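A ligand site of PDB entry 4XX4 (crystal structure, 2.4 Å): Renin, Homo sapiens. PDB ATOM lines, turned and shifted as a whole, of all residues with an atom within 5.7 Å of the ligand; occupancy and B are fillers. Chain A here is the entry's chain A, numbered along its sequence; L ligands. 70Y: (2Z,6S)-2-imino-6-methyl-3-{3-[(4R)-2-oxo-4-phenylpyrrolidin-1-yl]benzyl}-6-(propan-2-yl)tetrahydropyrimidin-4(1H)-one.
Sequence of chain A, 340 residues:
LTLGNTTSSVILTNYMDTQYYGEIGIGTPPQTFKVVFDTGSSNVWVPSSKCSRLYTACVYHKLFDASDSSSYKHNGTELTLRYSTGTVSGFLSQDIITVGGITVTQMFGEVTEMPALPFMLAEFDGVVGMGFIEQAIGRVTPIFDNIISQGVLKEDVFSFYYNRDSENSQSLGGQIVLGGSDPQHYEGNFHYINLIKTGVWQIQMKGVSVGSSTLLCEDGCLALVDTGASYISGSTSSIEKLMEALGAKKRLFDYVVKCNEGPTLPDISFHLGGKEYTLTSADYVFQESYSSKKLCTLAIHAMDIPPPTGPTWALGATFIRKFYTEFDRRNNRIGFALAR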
ATOM      1  N   THR A  18      24.232   9.293 -17.858  1.00  0.00           N
ATOM      2  CA  THR A  18      24.011   9.078 -19.292  1.00  0.00           C
ATOM      3  C   THR A  18      25.088   9.685 -20.191  1.00  0.00           C
ATOM      4  O   THR A  18      25.191   9.304 -21.354  1.00  0.00           O
ATOM      5  CB  THR A  18      22.593   9.566 -19.737  1.00  0.00           C
ATOM      6  OG1 THR A  18      22.462  10.969 -19.472  1.00  0.00           O
ATOM      7  CG2 THR A  18      21.445   8.804 -19.097  1.00  0.00           C
ATOM      8  N   GLN A  19      25.838  10.675 -19.686  1.00  0.00           N
ATOM      9  CA  GLN A  19      26.891  11.325 -20.474  1.00  0.00           C
ATOM     10  C   GLN A  19      28.133  11.452 -19.619  1.00  0.00           C
ATOM     11  O   GLN A  19      28.073  11.969 -18.499  1.00  0.00           O
ATOM     12  CB  GLN A  19      26.435  12.709 -20.989  1.00  0.00           C
ATOM     13  CG  GLN A  19      25.125  12.695 -21.801  1.00  0.00           C
ATOM     14  CD  GLN A  19      24.636  14.070 -22.171  1.00  0.00           C
ATOM     15  OE1 GLN A  19      25.423  14.966 -22.427  1.00  0.00           O
ATOM     16  NE2 GLN A  19      23.314  14.254 -22.256  1.00  0.00           N
ATOM     17  N   VAL A  36      33.084  13.354 -25.212  1.00  0.00           N
ATOM     18  CA  VAL A  36      32.804  11.953 -24.847  1.00  0.00           C
ATOM     19  C   VAL A  36      33.918  11.136 -25.524  1.00  0.00           C
ATOM     20  O   VAL A  36      34.202  11.356 -26.719  1.00  0.00           O
ATOM     21  CB  VAL A  36      31.410  11.489 -25.348  1.00  0.00           C
ATOM     22  CG1 VAL A  36      31.183   9.992 -25.116  1.00  0.00           C
ATOM     23  CG2 VAL A  36      30.302  12.297 -24.690  1.00  0.00           C
ATOM     24  N   ASP A  38      34.664   7.900 -26.967  1.00  0.00           N
ATOM     25  CA  ASP A  38      33.754   6.918 -27.523  1.00  0.00           C
ATOM     26  C   ASP A  38      34.379   5.758 -28.321  1.00  0.00           C
ATOM     27  O   ASP A  38      34.843   5.960 -29.428  1.00  0.00           O
ATOM     28  CB  ASP A  38      32.749   7.711 -28.399  1.00  0.00           C
ATOM     29  CG  ASP A  38      31.713   6.935 -29.143  1.00  0.00           C
ATOM     30  OD1 ASP A  38      31.276   5.884 -28.629  1.00  0.00           O
ATOM     31  OD2 ASP A  38      31.311   7.392 -30.211  1.00  0.00           O
ATOM     32  N   GLY A  40      32.665   3.369 -29.678  1.00  0.00           N
ATOM     33  CA  GLY A  40      31.736   3.072 -30.756  1.00  0.00           C
ATOM     34  C   GLY A  40      31.841   3.959 -31.996  1.00  0.00           C
ATOM     35  O   GLY A  40      30.957   3.908 -32.851  1.00  0.00           O
ATOM     36  N   SER A  41      32.884   4.814 -32.085  1.00  0.00           N
ATOM     37  CA  SER A  41      33.148   5.703 -33.234  1.00  0.00           C
ATOM     38  C   SER A  41      34.657   5.980 -33.313  1.00  0.00           C
ATOM     39  O   SER A  41      35.363   5.680 -32.351  1.00  0.00           O
ATOM     40  CB  SER A  41      32.316   6.986 -33.172  1.00  0.00           C
ATOM     41  OG  SER A  41      32.829   7.962 -32.283  1.00  0.00           O
ATOM     42  N   TRP A  45      35.554  15.231 -33.437  1.00  0.00           N
ATOM     43  CA  TRP A  45      34.819  16.384 -33.926  1.00  0.00           C
ATOM     44  C   TRP A  45      34.412  17.276 -32.771  1.00  0.00           C
ATOM     45  O   TRP A  45      34.160  16.789 -31.674  1.00  0.00           O
ATOM     46  CB  TRP A  45      33.602  16.010 -34.819  1.00  0.00           C
ATOM     47  CG  TRP A  45      32.444  15.362 -34.114  1.00  0.00           C
ATOM     48  CD1 TRP A  45      32.167  14.032 -34.066  1.00  0.00           C
ATOM     49  CD2 TRP A  45      31.362  16.024 -33.435  1.00  0.00           C
ATOM     50  NE1 TRP A  45      30.985  13.816 -33.387  1.00  0.00           N
ATOM     51  CE2 TRP A  45      30.480  15.022 -32.977  1.00  0.00           C
ATOM     52  CE3 TRP A  45      31.051  17.374 -33.156  1.00  0.00           C
ATOM     53  CZ2 TRP A  45      29.321  15.313 -32.248  1.00  0.00           C
ATOM     54  CZ3 TRP A  45      29.915  17.662 -32.420  1.00  0.00           C
ATOM     55  CH2 TRP A  45      29.060  16.643 -31.981  1.00  0.00           C
ATOM     56  N   TYR A  83      25.339   8.740 -37.149  1.00  0.00           N
ATOM     57  CA  TYR A  83      25.265   7.879 -35.979  1.00  0.00           C
ATOM     58  C   TYR A  83      23.826   7.401 -35.808  1.00  0.00           C
ATOM     59  O   TYR A  83      22.897   7.932 -36.428  1.00  0.00           O
ATOM     60  CB  TYR A  83      25.683   8.637 -34.688  1.00  0.00           C
ATOM     61  CG  TYR A  83      27.030   9.313 -34.693  1.00  0.00           C
ATOM     62  CD1 TYR A  83      28.210   8.569 -34.730  1.00  0.00           C
ATOM     63  CD2 TYR A  83      27.134  10.688 -34.527  1.00  0.00           C
ATOM     64  CE1 TYR A  83      29.452   9.200 -34.672  1.00  0.00           C
ATOM     65  CE2 TYR A  83      28.373  11.322 -34.483  1.00  0.00           C
ATOM     66  CZ  TYR A  83      29.537  10.577 -34.538  1.00  0.00           C
ATOM     67  OH  TYR A  83      30.752  11.210 -34.464  1.00  0.00           O
ATOM     68  N   SER A  84      23.632   6.445 -34.873  1.00  0.00           N
ATOM     69  CA  SER A  84      22.357   5.867 -34.503  1.00  0.00           C
ATOM     70  C   SER A  84      21.414   6.882 -33.805  1.00  0.00           C
ATOM     71  O   SER A  84      20.192   6.726 -33.829  1.00  0.00           O
ATOM     72  CB  SER A  84      22.602   4.674 -33.577  1.00  0.00           C
ATOM     73  OG  SER A  84      23.437   3.738 -34.237  1.00  0.00           O
ATOM     74  N   THR A  85      21.993   7.902 -33.159  1.00  0.00           N
ATOM     75  CA  THR A  85      21.208   8.881 -32.418  1.00  0.00           C
ATOM     76  C   THR A  85      20.932  10.177 -33.207  1.00  0.00           C
ATOM     77  O   THR A  85      20.066  10.986 -32.809  1.00  0.00           O
ATOM     78  CB  THR A  85      21.873   9.176 -31.052  1.00  0.00           C
ATOM     79  OG1 THR A  85      23.232   9.510 -31.285  1.00  0.00           O
ATOM     80  CG2 THR A  85      21.779   8.003 -30.106  1.00  0.00           C
ATOM     81  N   GLY A  86      21.655  10.354 -34.289  1.00  0.00           N
ATOM     82  CA  GLY A  86      21.568  11.530 -35.135  1.00  0.00           C
ATOM     83  C   GLY A  86      22.808  11.707 -35.994  1.00  0.00           C
ATOM     84  O   GLY A  86      23.742  10.905 -35.914  1.00  0.00           O
ATOM     85  N   PRO A 118      19.378  15.474 -31.471  1.00  0.00           N
ATOM     86  CA  PRO A 118      19.469  15.439 -30.000  1.00  0.00           C
ATOM     87  C   PRO A 118      20.450  16.396 -29.304  1.00  0.00           C
ATOM     88  O   PRO A 118      20.436  16.459 -28.079  1.00  0.00           O
ATOM     89  CB  PRO A 118      19.948  14.004 -29.757  1.00  0.00           C
ATOM     90  CG  PRO A 118      20.941  13.782 -30.890  1.00  0.00           C
ATOM     91  CD  PRO A 118      20.361  14.552 -32.079  1.00  0.00           C
ATOM     92  N   PHE A 119      21.308  17.114 -30.063  1.00  0.00           N
ATOM     93  CA  PHE A 119      22.439  17.878 -29.548  1.00  0.00           C
ATOM     94  C   PHE A 119      22.099  19.040 -28.581  1.00  0.00           C
ATOM     95  O   PHE A 119      23.008  19.471 -27.887  1.00  0.00           O
ATOM     96  CB  PHE A 119      23.366  18.319 -30.692  1.00  0.00           C
ATOM     97  CG  PHE A 119      23.978  17.084 -31.324  1.00  0.00           C
ATOM     98  CD1 PHE A 119      24.928  16.324 -30.644  1.00  0.00           C
ATOM     99  CD2 PHE A 119      23.519  16.609 -32.548  1.00  0.00           C
ATOM    100  CE1 PHE A 119      25.435  15.134 -31.195  1.00  0.00           C
ATOM    101  CE2 PHE A 119      24.016  15.419 -33.097  1.00  0.00           C
ATOM    102  CZ  PHE A 119      24.984  14.696 -32.419  1.00  0.00           C
ATOM    103  N   LEU A 121      20.328  18.388 -26.009  1.00  0.00           N
ATOM    104  CA  LEU A 121      20.316  17.565 -24.793  1.00  0.00           C
ATOM    105  C   LEU A 121      21.734  17.143 -24.375  1.00  0.00           C
ATOM    106  O   LEU A 121      21.925  16.572 -23.309  1.00  0.00           O
ATOM    107  CB  LEU A 121      19.425  16.324 -24.960  1.00  0.00           C
ATOM    108  CG  LEU A 121      17.902  16.572 -25.083  1.00  0.00           C
ATOM    109  CD1 LEU A 121      17.175  15.285 -25.417  1.00  0.00           C
ATOM    110  CD2 LEU A 121      17.305  17.141 -23.786  1.00  0.00           C
ATOM    111  N   ALA A 122      22.721  17.463 -25.213  1.00  0.00           N
ATOM    112  CA  ALA A 122      24.122  17.140 -24.946  1.00  0.00           C
ATOM    113  C   ALA A 122      24.790  18.175 -24.009  1.00  0.00           C
ATOM    114  O   ALA A 122      24.719  19.379 -24.258  1.00  0.00           O
ATOM    115  CB  ALA A 122      24.894  17.041 -26.255  1.00  0.00           C
ATOM    116  N   PHE A 124      28.091  17.763 -23.304  1.00  0.00           N
ATOM    117  CA  PHE A 124      29.366  17.781 -23.958  1.00  0.00           C
ATOM    118  C   PHE A 124      29.247  18.613 -25.232  1.00  0.00           C
ATOM    119  O   PHE A 124      28.133  18.840 -25.723  1.00  0.00           O
ATOM    120  CB  PHE A 124      29.806  16.318 -24.283  1.00  0.00           C
ATOM    121  CG  PHE A 124      28.872  15.534 -25.188  1.00  0.00           C
ATOM    122  CD1 PHE A 124      28.985  15.620 -26.583  1.00  0.00           C
ATOM    123  CD2 PHE A 124      27.873  14.719 -24.659  1.00  0.00           C
ATOM    124  CE1 PHE A 124      28.106  14.906 -27.424  1.00  0.00           C
ATOM    125  CE2 PHE A 124      27.007  14.002 -25.489  1.00  0.00           C
ATOM    126  CZ  PHE A 124      27.132  14.094 -26.879  1.00  0.00           C
ATOM    127  N   VAL A 127      33.062  14.900 -29.699  1.00  0.00           N
ATOM    128  CA  VAL A 127      33.364  13.466 -29.534  1.00  0.00           C
ATOM    129  C   VAL A 127      34.806  13.158 -29.915  1.00  0.00           C
ATOM    130  O   VAL A 127      35.305  13.677 -30.899  1.00  0.00           O
ATOM    131  CB  VAL A 127      32.344  12.594 -30.355  1.00  0.00           C
ATOM    132  CG1 VAL A 127      32.668  11.096 -30.276  1.00  0.00           C
ATOM    133  CG2 VAL A 127      30.890  12.850 -29.917  1.00  0.00           C
ATOM    134  N   ASP A 226      30.708  -0.254 -25.960  1.00  0.00           N
ATOM    135  CA  ASP A 226      30.520   1.142 -26.366  1.00  0.00           C
ATOM    136  C   ASP A 226      30.507   2.157 -25.222  1.00  0.00           C
ATOM    137  O   ASP A 226      29.495   2.317 -24.557  1.00  0.00           O
ATOM    138  CB  ASP A 226      29.218   1.222 -27.200  1.00  0.00           C
ATOM    139  CG  ASP A 226      28.999   2.480 -28.016  1.00  0.00           C
ATOM    140  OD1 ASP A 226      29.824   3.414 -27.899  1.00  0.00           O
ATOM    141  OD2 ASP A 226      27.996   2.538 -28.753  1.00  0.00           O
ATOM    142  N   GLY A 228      30.507   5.385 -25.505  1.00  0.00           N
ATOM    143  CA  GLY A 228      29.661   6.516 -25.908  1.00  0.00           C
ATOM    144  C   GLY A 228      28.186   6.260 -25.741  1.00  0.00           C
ATOM    145  O   GLY A 228      27.392   7.210 -25.729  1.00  0.00           O
ATOM    146  N   ALA A 229      27.779   4.986 -25.624  1.00  0.00           N
ATOM    147  CA  ALA A 229      26.376   4.637 -25.443  1.00  0.00           C
ATOM    148  C   ALA A 229      26.034   4.714 -23.937  1.00  0.00           C
ATOM    149  O   ALA A 229      26.792   4.248 -23.090  1.00  0.00           O
ATOM    150  CB  ALA A 229      26.111   3.247 -25.978  1.00  0.00           C
ATOM    151  N   SER A 230      24.899   5.321 -23.616  1.00  0.00           N
ATOM    152  CA  SER A 230      24.419   5.489 -22.250  1.00  0.00           C
ATOM    153  C   SER A 230      23.929   4.186 -21.645  1.00  0.00           C
ATOM    154  O   SER A 230      24.082   3.982 -20.444  1.00  0.00           O
ATOM    155  CB  SER A 230      23.221   6.437 -22.236  1.00  0.00           C
ATOM    156  OG  SER A 230      23.578   7.692 -22.770  1.00  0.00           O
ATOM    157  N   TYR A 231      23.239   3.389 -22.457  1.00  0.00           N
ATOM    158  CA  TYR A 231      22.541   2.217 -21.976  1.00  0.00           C
ATOM    159  C   TYR A 231      23.054   0.945 -22.598  1.00  0.00           C
ATOM    160  O   TYR A 231      23.909   0.960 -23.496  1.00  0.00           O
ATOM    161  CB  TYR A 231      21.024   2.377 -22.285  1.00  0.00           C
ATOM    162  CG  TYR A 231      20.452   3.748 -21.970  1.00  0.00           C
ATOM    163  CD1 TYR A 231      20.264   4.170 -20.657  1.00  0.00           C
ATOM    164  CD2 TYR A 231      20.157   4.655 -22.997  1.00  0.00           C
ATOM    165  CE1 TYR A 231      19.754   5.437 -20.365  1.00  0.00           C
ATOM    166  CE2 TYR A 231      19.667   5.937 -22.708  1.00  0.00           C
ATOM    167  CZ  TYR A 231      19.470   6.322 -21.395  1.00  0.00           C
ATOM    168  OH  TYR A 231      19.016   7.588 -21.127  1.00  0.00           O
ATOM    169  N   MET A 303      17.690  -0.946 -29.888  1.00  0.00           N
ATOM    170  CA  MET A 303      18.489  -0.206 -30.860  1.00  0.00           C
ATOM    171  C   MET A 303      18.895  -1.171 -31.960  1.00  0.00           C
ATOM    172  O   MET A 303      19.637  -2.128 -31.707  1.00  0.00           O
ATOM    173  CB  MET A 303      19.718   0.450 -30.198  1.00  0.00           C
ATOM    174  CG  MET A 303      20.649   1.153 -31.119  1.00  0.00           C
ATOM    175  SD  MET A 303      20.055   2.786 -31.548  1.00  0.00           S
ATOM    176  CE  MET A 303      20.421   3.713 -29.989  1.00  0.00           C
HETATM  177  C25 70Y L   1      23.797  11.838 -27.639  1.00  0.00           C
HETATM  178  C26 70Y L   1      23.354  12.960 -28.320  1.00  0.00           C
HETATM  179  C27 70Y L   1      22.762  13.978 -27.625  1.00  0.00           C
HETATM  180  C28 70Y L   1      22.589  13.887 -26.259  1.00  0.00           C
HETATM  181  C31 70Y L   1      26.740  10.892 -29.559  1.00  0.00           C
HETATM  182  C29 70Y L   1      23.041  12.775 -25.585  1.00  0.00           C
HETATM  183  C24 70Y L   1      23.659  11.736 -26.263  1.00  0.00           C
HETATM  184  C23 70Y L   1      24.664   9.367 -26.324  1.00  0.00           C
HETATM  185  C22 70Y L   1      24.155  10.529 -25.483  1.00  0.00           C
HETATM  186  C20 70Y L   1      22.516   8.823 -25.532  1.00  0.00           C
HETATM  187  C4  70Y L   1      26.000   7.138 -30.974  1.00  0.00           C
HETATM  188  C2  70Y L   1      27.936   8.680 -30.256  1.00  0.00           C
HETATM  189  C3  70Y L   1      26.870   8.325 -31.279  1.00  0.00           C
HETATM  190  C11 70Y L   1      29.037   9.361 -31.050  1.00  0.00           C
HETATM  191  C17 70Y L   1      22.680   4.997 -27.342  1.00  0.00           C
HETATM  192  C16 70Y L   1      22.689   6.203 -26.685  1.00  0.00           C
HETATM  193  C15 70Y L   1      23.662   7.157 -26.971  1.00  0.00           C
HETATM  194  C14 70Y L   1      24.646   6.854 -27.888  1.00  0.00           C
HETATM  195  C12 70Y L   1      28.337   9.857 -27.976  1.00  0.00           C
HETATM  196  N1  70Y L   1      28.516   7.449 -29.743  1.00  0.00           N
HETATM  197  N5  70Y L   1      26.534   6.220 -30.102  1.00  0.00           N
HETATM  198  C6  70Y L   1      27.902   6.222 -29.843  1.00  0.00           C
HETATM  199  N7  70Y L   1      28.540   5.103 -29.742  1.00  0.00           N
HETATM  200  O8  70Y L   1      24.894   7.040 -31.510  1.00  0.00           O
HETATM  201  C9  70Y L   1      25.681   5.184 -29.547  1.00  0.00           C
HETATM  202  C10 70Y L   1      27.389   9.578 -29.119  1.00  0.00           C
HETATM  203  C13 70Y L   1      24.658   5.627 -28.549  1.00  0.00           C
HETATM  204  C18 70Y L   1      23.659   4.720 -28.274  1.00  0.00           C
HETATM  205  N19 70Y L   1      23.614   8.384 -26.253  1.00  0.00           N
HETATM  206  C21 70Y L   1      22.992   9.969 -24.699  1.00  0.00           C
HETATM  207  O30 70Y L   1      21.343   8.442 -25.541  1.00  0.00           O
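Gln 19 touches the ligand.
CA of Gly 40 touches N7 of the ligand, 3.9 Å away.
Tyr 83 touches the ligand.
Ser 84 touches the ligand (N to O8, 3.6 Å).
O of Pro 118 touches C27 of the ligand, 3.4 Å away.
Leu 121 touches the ligand (C to C28, 3.9 Å).
N of Ala 122 touches C28 of the ligand (3.7 Å).
O of Gly 228 touches C14 of the ligand, at 3.5 Å.
Ala 229 touches the ligand (CB to C18, 3.7 Å).
OG of Ser 230 touches C21 of the ligand, 3.0 Å away.
Met 303 touches the ligand (CE to C17, 3.7 Å).
Hydrophobic or aromatic side chains that line the ligand: Tyr 83, Pro 118, Ala 122, Ala 229 and Met 303.
Within 4 Å of the ligand: Gln 19, Asp 38, Gly 40, Tyr 83, Ser 84, Thr 85, Pro 118, Leu 121, Ala 122, Asp 226, Gly 228, Ala 229, Ser 230 and Met 303.
The nearest printed residue that does not touch the ligand is Val 36 (4.04 Å).
The side-chain carboxylate of Asp 226 sits at hydrogen-bond distance from a nitrogen (N7) of the ligand, at 2.8 Å.
The side-chain carboxylate of Asp 38 is in hydrogen-bond range of a nitrogen (N1) of the ligand, at 2.8 Å.
An oxygen (O8) of the ligand is in hydrogen-bond range of the backbone NH of Thr 85 (3.4 Å).
The side-chain hydroxyl (OG1) of Thr 85 sits at hydrogen-bond distance from an oxygen (O8) of the ligand, at 3.0 Å.
OD1 of Asp 226 lies within hydrogen-bond range of N of Gly 228 (3.2 Å).
The side-chain carboxylate (OD1) of Asp 226 lies within hydrogen-bond range of the backbone NH (N) of Gly 40.
N of Gly 228 sits close to OD1 of Asp 38, 3.3 Å away.
OD1 of Asp 38 sits at hydrogen-bond distance from N of Gly 40 (3.1 Å).
OD2 of Asp 38 is in hydrogen-bond range of OG of Ser 41 (2.6 Å).
The side-chain hydroxyl of Ser 230 is in hydrogen-bond range of the backbone carbonyl oxygen of Thr 18, 2.7 Å away.
The side-chain hydroxyl (OH) of Tyr 83 sits at hydrogen-bond distance from the indole nitrogen (NE1) of Trp 45 (2.8 Å).
The side-chain amide nitrogen of Gln 19 lies within hydrogen-bond range of the backbone carbonyl oxygen of Leu 121.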
